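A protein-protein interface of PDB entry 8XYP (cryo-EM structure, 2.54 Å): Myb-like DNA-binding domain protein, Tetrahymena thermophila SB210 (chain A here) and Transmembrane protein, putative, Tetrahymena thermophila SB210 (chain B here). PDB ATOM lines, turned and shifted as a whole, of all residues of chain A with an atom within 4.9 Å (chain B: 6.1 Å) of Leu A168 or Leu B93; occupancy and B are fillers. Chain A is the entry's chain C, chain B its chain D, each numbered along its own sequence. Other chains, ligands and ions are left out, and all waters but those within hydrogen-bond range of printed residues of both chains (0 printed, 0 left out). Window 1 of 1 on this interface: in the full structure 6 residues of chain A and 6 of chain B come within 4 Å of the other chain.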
ATOM      1  N   THR A 166      -3.970 -22.761  18.640  1.00  0.00           N
ATOM      2  CA  THR A 166      -3.872 -24.186  18.369  1.00  0.00           C
ATOM      3  C   THR A 166      -3.399 -24.427  16.938  1.00  0.00           C
ATOM      4  O   THR A 166      -3.374 -23.519  16.104  1.00  0.00           O
ATOM      5  CB  THR A 166      -5.220 -24.875  18.591  1.00  0.00           C
ATOM      6  OG1 THR A 166      -6.020 -24.757  17.408  1.00  0.00           O
ATOM      7  CG2 THR A 166      -5.955 -24.247  19.766  1.00  0.00           C
ATOM      8  N   ASN A 167      -3.019 -25.679  16.661  1.00  0.00           N
ATOM      9  CA  ASN A 167      -2.502 -26.030  15.341  1.00  0.00           C
ATOM     10  C   ASN A 167      -3.546 -25.837  14.249  1.00  0.00           C
ATOM     11  O   ASN A 167      -3.198 -25.506  13.111  1.00  0.00           O
ATOM     12  CB  ASN A 167      -2.005 -27.477  15.338  1.00  0.00           C
ATOM     13  CG  ASN A 167      -0.857 -27.704  16.301  1.00  0.00           C
ATOM     14  OD1 ASN A 167      -0.826 -28.699  17.023  1.00  0.00           O
ATOM     15  ND2 ASN A 167       0.096 -26.780  16.314  1.00  0.00           N
ATOM     16  N   LEU A 168      -4.826 -26.028  14.578  1.00  0.00           N
ATOM     17  CA  LEU A 168      -5.880 -25.868  13.581  1.00  0.00           C
ATOM     18  C   LEU A 168      -6.038 -24.411  13.165  1.00  0.00           C
ATOM     19  O   LEU A 168      -6.086 -24.103  11.970  1.00  0.00           O
ATOM     20  CB  LEU A 168      -7.201 -26.413  14.118  1.00  0.00           C
ATOM     21  CG  LEU A 168      -8.325 -26.565  13.093  1.00  0.00           C
ATOM     22  CD1 LEU A 168      -7.814 -27.120  11.768  1.00  0.00           C
ATOM     23  CD2 LEU A 168      -9.422 -27.436  13.657  1.00  0.00           C
ATOM     24  N   GLU A 169      -6.126 -23.497  14.135  1.00  0.00           N
ATOM     25  CA  GLU A 169      -6.263 -22.089  13.778  1.00  0.00           C
ATOM     26  C   GLU A 169      -4.975 -21.533  13.189  1.00  0.00           C
ATOM     27  O   GLU A 169      -5.023 -20.655  12.319  1.00  0.00           O
ATOM     28  CB  GLU A 169      -6.718 -21.267  14.983  1.00  0.00           C
ATOM     29  CG  GLU A 169      -6.004 -21.564  16.278  1.00  0.00           C
ATOM     30  CD  GLU A 169      -6.889 -21.311  17.483  1.00  0.00           C
ATOM     31  OE1 GLU A 169      -8.125 -21.267  17.311  1.00  0.00           O
ATOM     32  OE2 GLU A 169      -6.354 -21.153  18.599  1.00  0.00           O
ATOM     33  N   ILE A 170      -3.823 -22.057  13.618  1.00  0.00           N
ATOM     34  CA  ILE A 170      -2.556 -21.705  12.983  1.00  0.00           C
ATOM     35  C   ILE A 170      -2.580 -22.100  11.511  1.00  0.00           C
ATOM     36  O   ILE A 170      -2.203 -21.315  10.635  1.00  0.00           O
ATOM     37  CB  ILE A 170      -1.381 -22.362  13.731  1.00  0.00           C
ATOM     38  CG1 ILE A 170      -1.032 -21.564  14.987  1.00  0.00           C
ATOM     39  CG2 ILE A 170      -0.159 -22.474  12.843  1.00  0.00           C
ATOM     40  CD1 ILE A 170       0.092 -22.166  15.800  1.00  0.00           C
ATOM     41  N   LEU A 171      -3.062 -23.310  11.214  1.00  0.00           N
ATOM     42  CA  LEU A 171      -3.114 -23.769   9.830  1.00  0.00           C
ATOM     43  C   LEU A 171      -4.148 -23.009   9.007  1.00  0.00           C
ATOM     44  O   LEU A 171      -3.928 -22.777   7.813  1.00  0.00           O
ATOM     45  CB  LEU A 171      -3.388 -25.269   9.788  1.00  0.00           C
ATOM     46  CG  LEU A 171      -2.122 -26.119   9.883  1.00  0.00           C
ATOM     47  CD1 LEU A 171      -2.423 -27.472  10.489  1.00  0.00           C
ATOM     48  CD2 LEU A 171      -1.490 -26.272   8.512  1.00  0.00           C
ATOM     49  N   THR A 172      -5.274 -22.615   9.612  1.00  0.00           N
ATOM     50  CA  THR A 172      -6.228 -21.773   8.890  1.00  0.00           C
ATOM     51  C   THR A 172      -5.618 -20.419   8.561  1.00  0.00           C
ATOM     52  O   THR A 172      -5.826 -19.884   7.466  1.00  0.00           O
ATOM     53  CB  THR A 172      -7.519 -21.575   9.689  1.00  0.00           C
ATOM     54  OG1 THR A 172      -7.224 -20.940  10.937  1.00  0.00           O
ATOM     55  CG2 THR A 172      -8.233 -22.893   9.928  1.00  0.00           C
ATOM     56  N   GLN B  52     -14.751 -26.382  18.486  1.00  0.00           N
ATOM     57  CA  GLN B  52     -14.145 -27.163  17.404  1.00  0.00           C
ATOM     58  C   GLN B  52     -13.685 -28.494  17.996  1.00  0.00           C
ATOM     59  O   GLN B  52     -12.568 -28.605  18.505  1.00  0.00           O
ATOM     60  CB  GLN B  52     -12.998 -26.404  16.750  1.00  0.00           C
ATOM     61  CG  GLN B  52     -12.249 -25.467  17.686  1.00  0.00           C
ATOM     62  CD  GLN B  52     -11.019 -24.863  17.038  1.00  0.00           C
ATOM     63  OE1 GLN B  52     -10.952 -24.724  15.817  1.00  0.00           O
ATOM     64  NE2 GLN B  52     -10.037 -24.501  17.854  1.00  0.00           N
ATOM     65  N   ASN B  87     -14.648 -25.452   9.282  1.00  0.00           N
ATOM     66  CA  ASN B  87     -13.470 -24.895   8.631  1.00  0.00           C
ATOM     67  C   ASN B  87     -13.163 -25.706   7.382  1.00  0.00           C
ATOM     68  O   ASN B  87     -13.083 -26.936   7.440  1.00  0.00           O
ATOM     69  CB  ASN B  87     -12.269 -24.906   9.572  1.00  0.00           C
ATOM     70  CG  ASN B  87     -12.340 -23.829  10.627  1.00  0.00           C
ATOM     71  OD1 ASN B  87     -13.007 -22.810  10.448  1.00  0.00           O
ATOM     72  ND2 ASN B  87     -11.643 -24.044  11.737  1.00  0.00           N
ATOM     73  N   ILE B  88     -12.997 -25.016   6.251  1.00  0.00           N
ATOM     74  CA  ILE B  88     -12.545 -25.658   5.023  1.00  0.00           C
ATOM     75  C   ILE B  88     -11.165 -26.271   5.183  1.00  0.00           C
ATOM     76  O   ILE B  88     -10.913 -27.379   4.681  1.00  0.00           O
ATOM     77  CB  ILE B  88     -12.579 -24.615   3.886  1.00  0.00           C
ATOM     78  CG1 ILE B  88     -14.017 -24.147   3.651  1.00  0.00           C
ATOM     79  CG2 ILE B  88     -11.953 -25.152   2.609  1.00  0.00           C
ATOM     80  CD1 ILE B  88     -15.004 -25.277   3.457  1.00  0.00           C
ATOM     81  N   VAL B  89     -10.282 -25.579   5.902  1.00  0.00           N
ATOM     82  CA  VAL B  89      -8.964 -26.116   6.213  1.00  0.00           C
ATOM     83  C   VAL B  89      -9.092 -27.400   7.019  1.00  0.00           C
ATOM     84  O   VAL B  89      -8.421 -28.395   6.730  1.00  0.00           O
ATOM     85  CB  VAL B  89      -8.131 -25.062   6.962  1.00  0.00           C
ATOM     86  CG1 VAL B  89      -6.821 -25.655   7.455  1.00  0.00           C
ATOM     87  CG2 VAL B  89      -7.891 -23.857   6.077  1.00  0.00           C
ATOM     88  N   GLU B  90      -9.965 -27.404   8.031  1.00  0.00           N
ATOM     89  CA  GLU B  90     -10.150 -28.603   8.841  1.00  0.00           C
ATOM     90  C   GLU B  90     -10.754 -29.746   8.033  1.00  0.00           C
ATOM     91  O   GLU B  90     -10.366 -30.898   8.226  1.00  0.00           O
ATOM     92  CB  GLU B  90     -11.015 -28.299  10.065  1.00  0.00           C
ATOM     93  CG  GLU B  90     -11.240 -29.495  10.976  1.00  0.00           C
ATOM     94  CD  GLU B  90     -12.123 -29.171  12.160  1.00  0.00           C
ATOM     95  OE1 GLU B  90     -13.131 -28.461  11.973  1.00  0.00           O
ATOM     96  OE2 GLU B  90     -11.814 -29.640  13.277  1.00  0.00           O
ATOM     97  N   LEU B  91     -11.695 -29.452   7.130  1.00  0.00           N
ATOM     98  CA  LEU B  91     -12.223 -30.485   6.244  1.00  0.00           C
ATOM     99  C   LEU B  91     -11.134 -31.105   5.381  1.00  0.00           C
ATOM    100  O   LEU B  91     -11.066 -32.337   5.274  1.00  0.00           O
ATOM    101  CB  LEU B  91     -13.317 -29.911   5.340  1.00  0.00           C
ATOM    102  CG  LEU B  91     -14.627 -29.407   5.950  1.00  0.00           C
ATOM    103  CD1 LEU B  91     -15.739 -29.482   4.925  1.00  0.00           C
ATOM    104  CD2 LEU B  91     -15.001 -30.188   7.187  1.00  0.00           C
ATOM    105  N   GLU B  92     -10.262 -30.283   4.798  1.00  0.00           N
ATOM    106  CA  GLU B  92      -9.118 -30.776   4.039  1.00  0.00           C
ATOM    107  C   GLU B  92      -8.152 -31.591   4.891  1.00  0.00           C
ATOM    108  O   GLU B  92      -7.652 -32.622   4.437  1.00  0.00           O
ATOM    109  CB  GLU B  92      -8.367 -29.606   3.394  1.00  0.00           C
ATOM    110  CG  GLU B  92      -7.166 -30.018   2.559  1.00  0.00           C
ATOM    111  CD  GLU B  92      -6.451 -28.834   1.942  1.00  0.00           C
ATOM    112  OE1 GLU B  92      -6.822 -27.685   2.259  1.00  0.00           O
ATOM    113  OE2 GLU B  92      -5.522 -29.052   1.137  1.00  0.00           O
ATOM    114  N   LEU B  93      -7.895 -31.153   6.125  1.00  0.00           N
ATOM    115  CA  LEU B  93      -6.989 -31.878   7.012  1.00  0.00           C
ATOM    116  C   LEU B  93      -7.555 -33.236   7.407  1.00  0.00           C
ATOM    117  O   LEU B  93      -6.828 -34.237   7.437  1.00  0.00           O
ATOM    118  CB  LEU B  93      -6.705 -31.034   8.254  1.00  0.00           C
ATOM    119  CG  LEU B  93      -5.882 -29.765   8.036  1.00  0.00           C
ATOM    120  CD1 LEU B  93      -5.461 -29.158   9.353  1.00  0.00           C
ATOM    121  CD2 LEU B  93      -4.674 -30.064   7.182  1.00  0.00           C
ATOM    122  N   ARG B  94      -8.848 -33.291   7.721  1.00  0.00           N
ATOM    123  CA  ARG B  94      -9.494 -34.547   8.077  1.00  0.00           C
ATOM    124  C   ARG B  94      -9.507 -35.491   6.882  1.00  0.00           C
ATOM    125  O   ARG B  94      -9.288 -36.697   7.039  1.00  0.00           O
ATOM    126  CB  ARG B  94     -10.918 -34.306   8.587  1.00  0.00           C
ATOM    127  CG  ARG B  94     -11.019 -33.468   9.855  1.00  0.00           C
ATOM    128  CD  ARG B  94     -10.462 -34.153  11.079  1.00  0.00           C
ATOM    129  NE  ARG B  94     -10.477 -33.261  12.232  1.00  0.00           N
ATOM    130  CZ  ARG B  94     -10.066 -33.595  13.446  1.00  0.00           C
ATOM    131  NH1 ARG B  94      -9.612 -34.806  13.714  1.00  0.00           N
ATOM    132  NH2 ARG B  94     -10.113 -32.689  14.419  1.00  0.00           N
ATOM    133  N   THR B  95      -9.750 -34.954   5.684  1.00  0.00           N
ATOM    134  CA  THR B  95      -9.692 -35.759   4.469  1.00  0.00           C
ATOM    135  C   THR B  95      -8.283 -36.289   4.222  1.00  0.00           C
ATOM    136  O   THR B  95      -8.114 -37.412   3.740  1.00  0.00           O
ATOM    137  CB  THR B  95     -10.172 -34.945   3.268  1.00  0.00           C
ATOM    138  OG1 THR B  95     -11.358 -34.228   3.627  1.00  0.00           O
ATOM    139  CG2 THR B  95     -10.473 -35.856   2.090  1.00  0.00           C
ATOM    140  N   CYS B  96      -7.269 -35.480   4.543  1.00  0.00           N
ATOM    141  CA  CYS B  96      -5.888 -35.953   4.484  1.00  0.00           C
ATOM    142  C   CYS B  96      -5.657 -37.101   5.458  1.00  0.00           C
ATOM    143  O   CYS B  96      -4.964 -38.072   5.133  1.00  0.00           O
ATOM    144  CB  CYS B  96      -4.924 -34.810   4.800  1.00  0.00           C
ATOM    145  SG  CYS B  96      -4.583 -33.660   3.464  1.00  0.00           S
ATOM    146  N   MET B  97      -6.207 -36.989   6.669  1.00  0.00           N
ATOM    147  CA  MET B  97      -6.026 -38.035   7.671  1.00  0.00           C
ATOM    148  C   MET B  97      -6.695 -39.337   7.247  1.00  0.00           C
ATOM    149  O   MET B  97      -6.142 -40.424   7.444  1.00  0.00           O
ATOM    150  CB  MET B  97      -6.568 -37.577   9.023  1.00  0.00           C
ATOM    151  CG  MET B  97      -5.525 -36.948   9.918  1.00  0.00           C
ATOM    152  SD  MET B  97      -6.232 -35.728  11.032  1.00  0.00           S
ATOM    153  CE  MET B  97      -7.735 -36.567  11.509  1.00  0.00           C
ATOM    154  N   ILE B  98      -7.895 -39.248   6.663  1.00  0.00           N
ATOM    155  CA  ILE B  98      -8.612 -40.459   6.265  1.00  0.00           C
ATOM    156  C   ILE B  98      -8.167 -40.998   4.916  1.00  0.00           C
ATOM    157  O   ILE B  98      -8.652 -42.056   4.496  1.00  0.00           O
ATOM    158  CB  ILE B  98     -10.137 -40.238   6.233  1.00  0.00           C
ATOM    159  CG1 ILE B  98     -10.537 -39.371   5.044  1.00  0.00           C
ATOM    160  CG2 ILE B  98     -10.612 -39.615   7.528  1.00  0.00           C
ATOM    161  CD1 ILE B  98     -12.020 -39.363   4.795  1.00  0.00           C
ATOM    162  N   ILE B 104      -3.197 -34.142  -0.476  1.00  0.00           N
ATOM    163  CA  ILE B 104      -4.146 -34.889  -1.294  1.00  0.00           C
ATOM    164  C   ILE B 104      -4.317 -34.181  -2.634  1.00  0.00           C
ATOM    165  O   ILE B 104      -5.216 -33.352  -2.813  1.00  0.00           O
ATOM    166  CB  ILE B 104      -5.494 -35.078  -0.571  1.00  0.00           C
ATOM    167  CG1 ILE B 104      -5.918 -33.806   0.173  1.00  0.00           C
ATOM    168  CG2 ILE B 104      -5.410 -36.248   0.396  1.00  0.00           C
ATOM    169  CD1 ILE B 104      -7.200 -33.957   0.961  1.00  0.00           C
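The backbone carbonyl oxygen of Glu A169 sits at hydrogen-bond distance from the side-chain hydroxyl of Thr A172, at 2.6 Å. OE2 of Glu A169 sits at hydrogen-bond distance from N of Thr A166, 2.9 Å away. OG1 of Thr A166 lies close to N of Leu A168 (3.3 Å). OE2 of Glu B90 lies within salt-bridge range of NH2 of Arg B94 (3.7 Å).
CD2 of Leu A168 touches OE1 of Gln B52, 3.8 Å away. Glu B90 touches Leu A168. Leu B93 touches Leu A168. NE2 of Gln B52 touches OE1 of Glu A169 (3.8 Å). CD1 of Leu A171 touches CD1 of Leu B93 (3.7 Å). CB of Val B89 touches CG2 of Thr A172 (3.7 Å).
Of chain B, only Gln B52, Glu B90 and Leu B93 come within 4 Å of Leu A168. Of chain A, only Leu A168 and Leu A171 come within 4 Å of Leu B93. Printed residues of chain A within 4 Å of Gln B52: Leu A168 and Glu A169. Of the printed residues of chain A, Glu B90 touches Leu A168. Of the printed residues of chain B, Thr A172 touches Val B89 (3.7 Å). Of the printed residues of chain A, Val B89 touches Thr A172 (3.7 Å). Of the printed residues of chain B, Leu A171 touches Leu B93. The nearest residue of chain B that does not touch Leu A168 is Asn B87 (4.4 Å). The nearest printed residue of chain A that does not touch Leu B93 is Asn A167 (5.7 Å).
Of the 7 printed residues of chain A, 4 touch a printed residue of chain B. Hydrophobic or aromatic side chains of chain A within 4 Å of the printed part of chain B: Leu A168 and Leu A171. Printed residues of chain B that touch a printed residue of chain A: Gln B52, Val B89, Glu B90 and Leu B93. Among the printed residues, no Asp or Glu carboxylate lies within 4 Å of a Lys or Arg side-chain nitrogen of the other chain.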
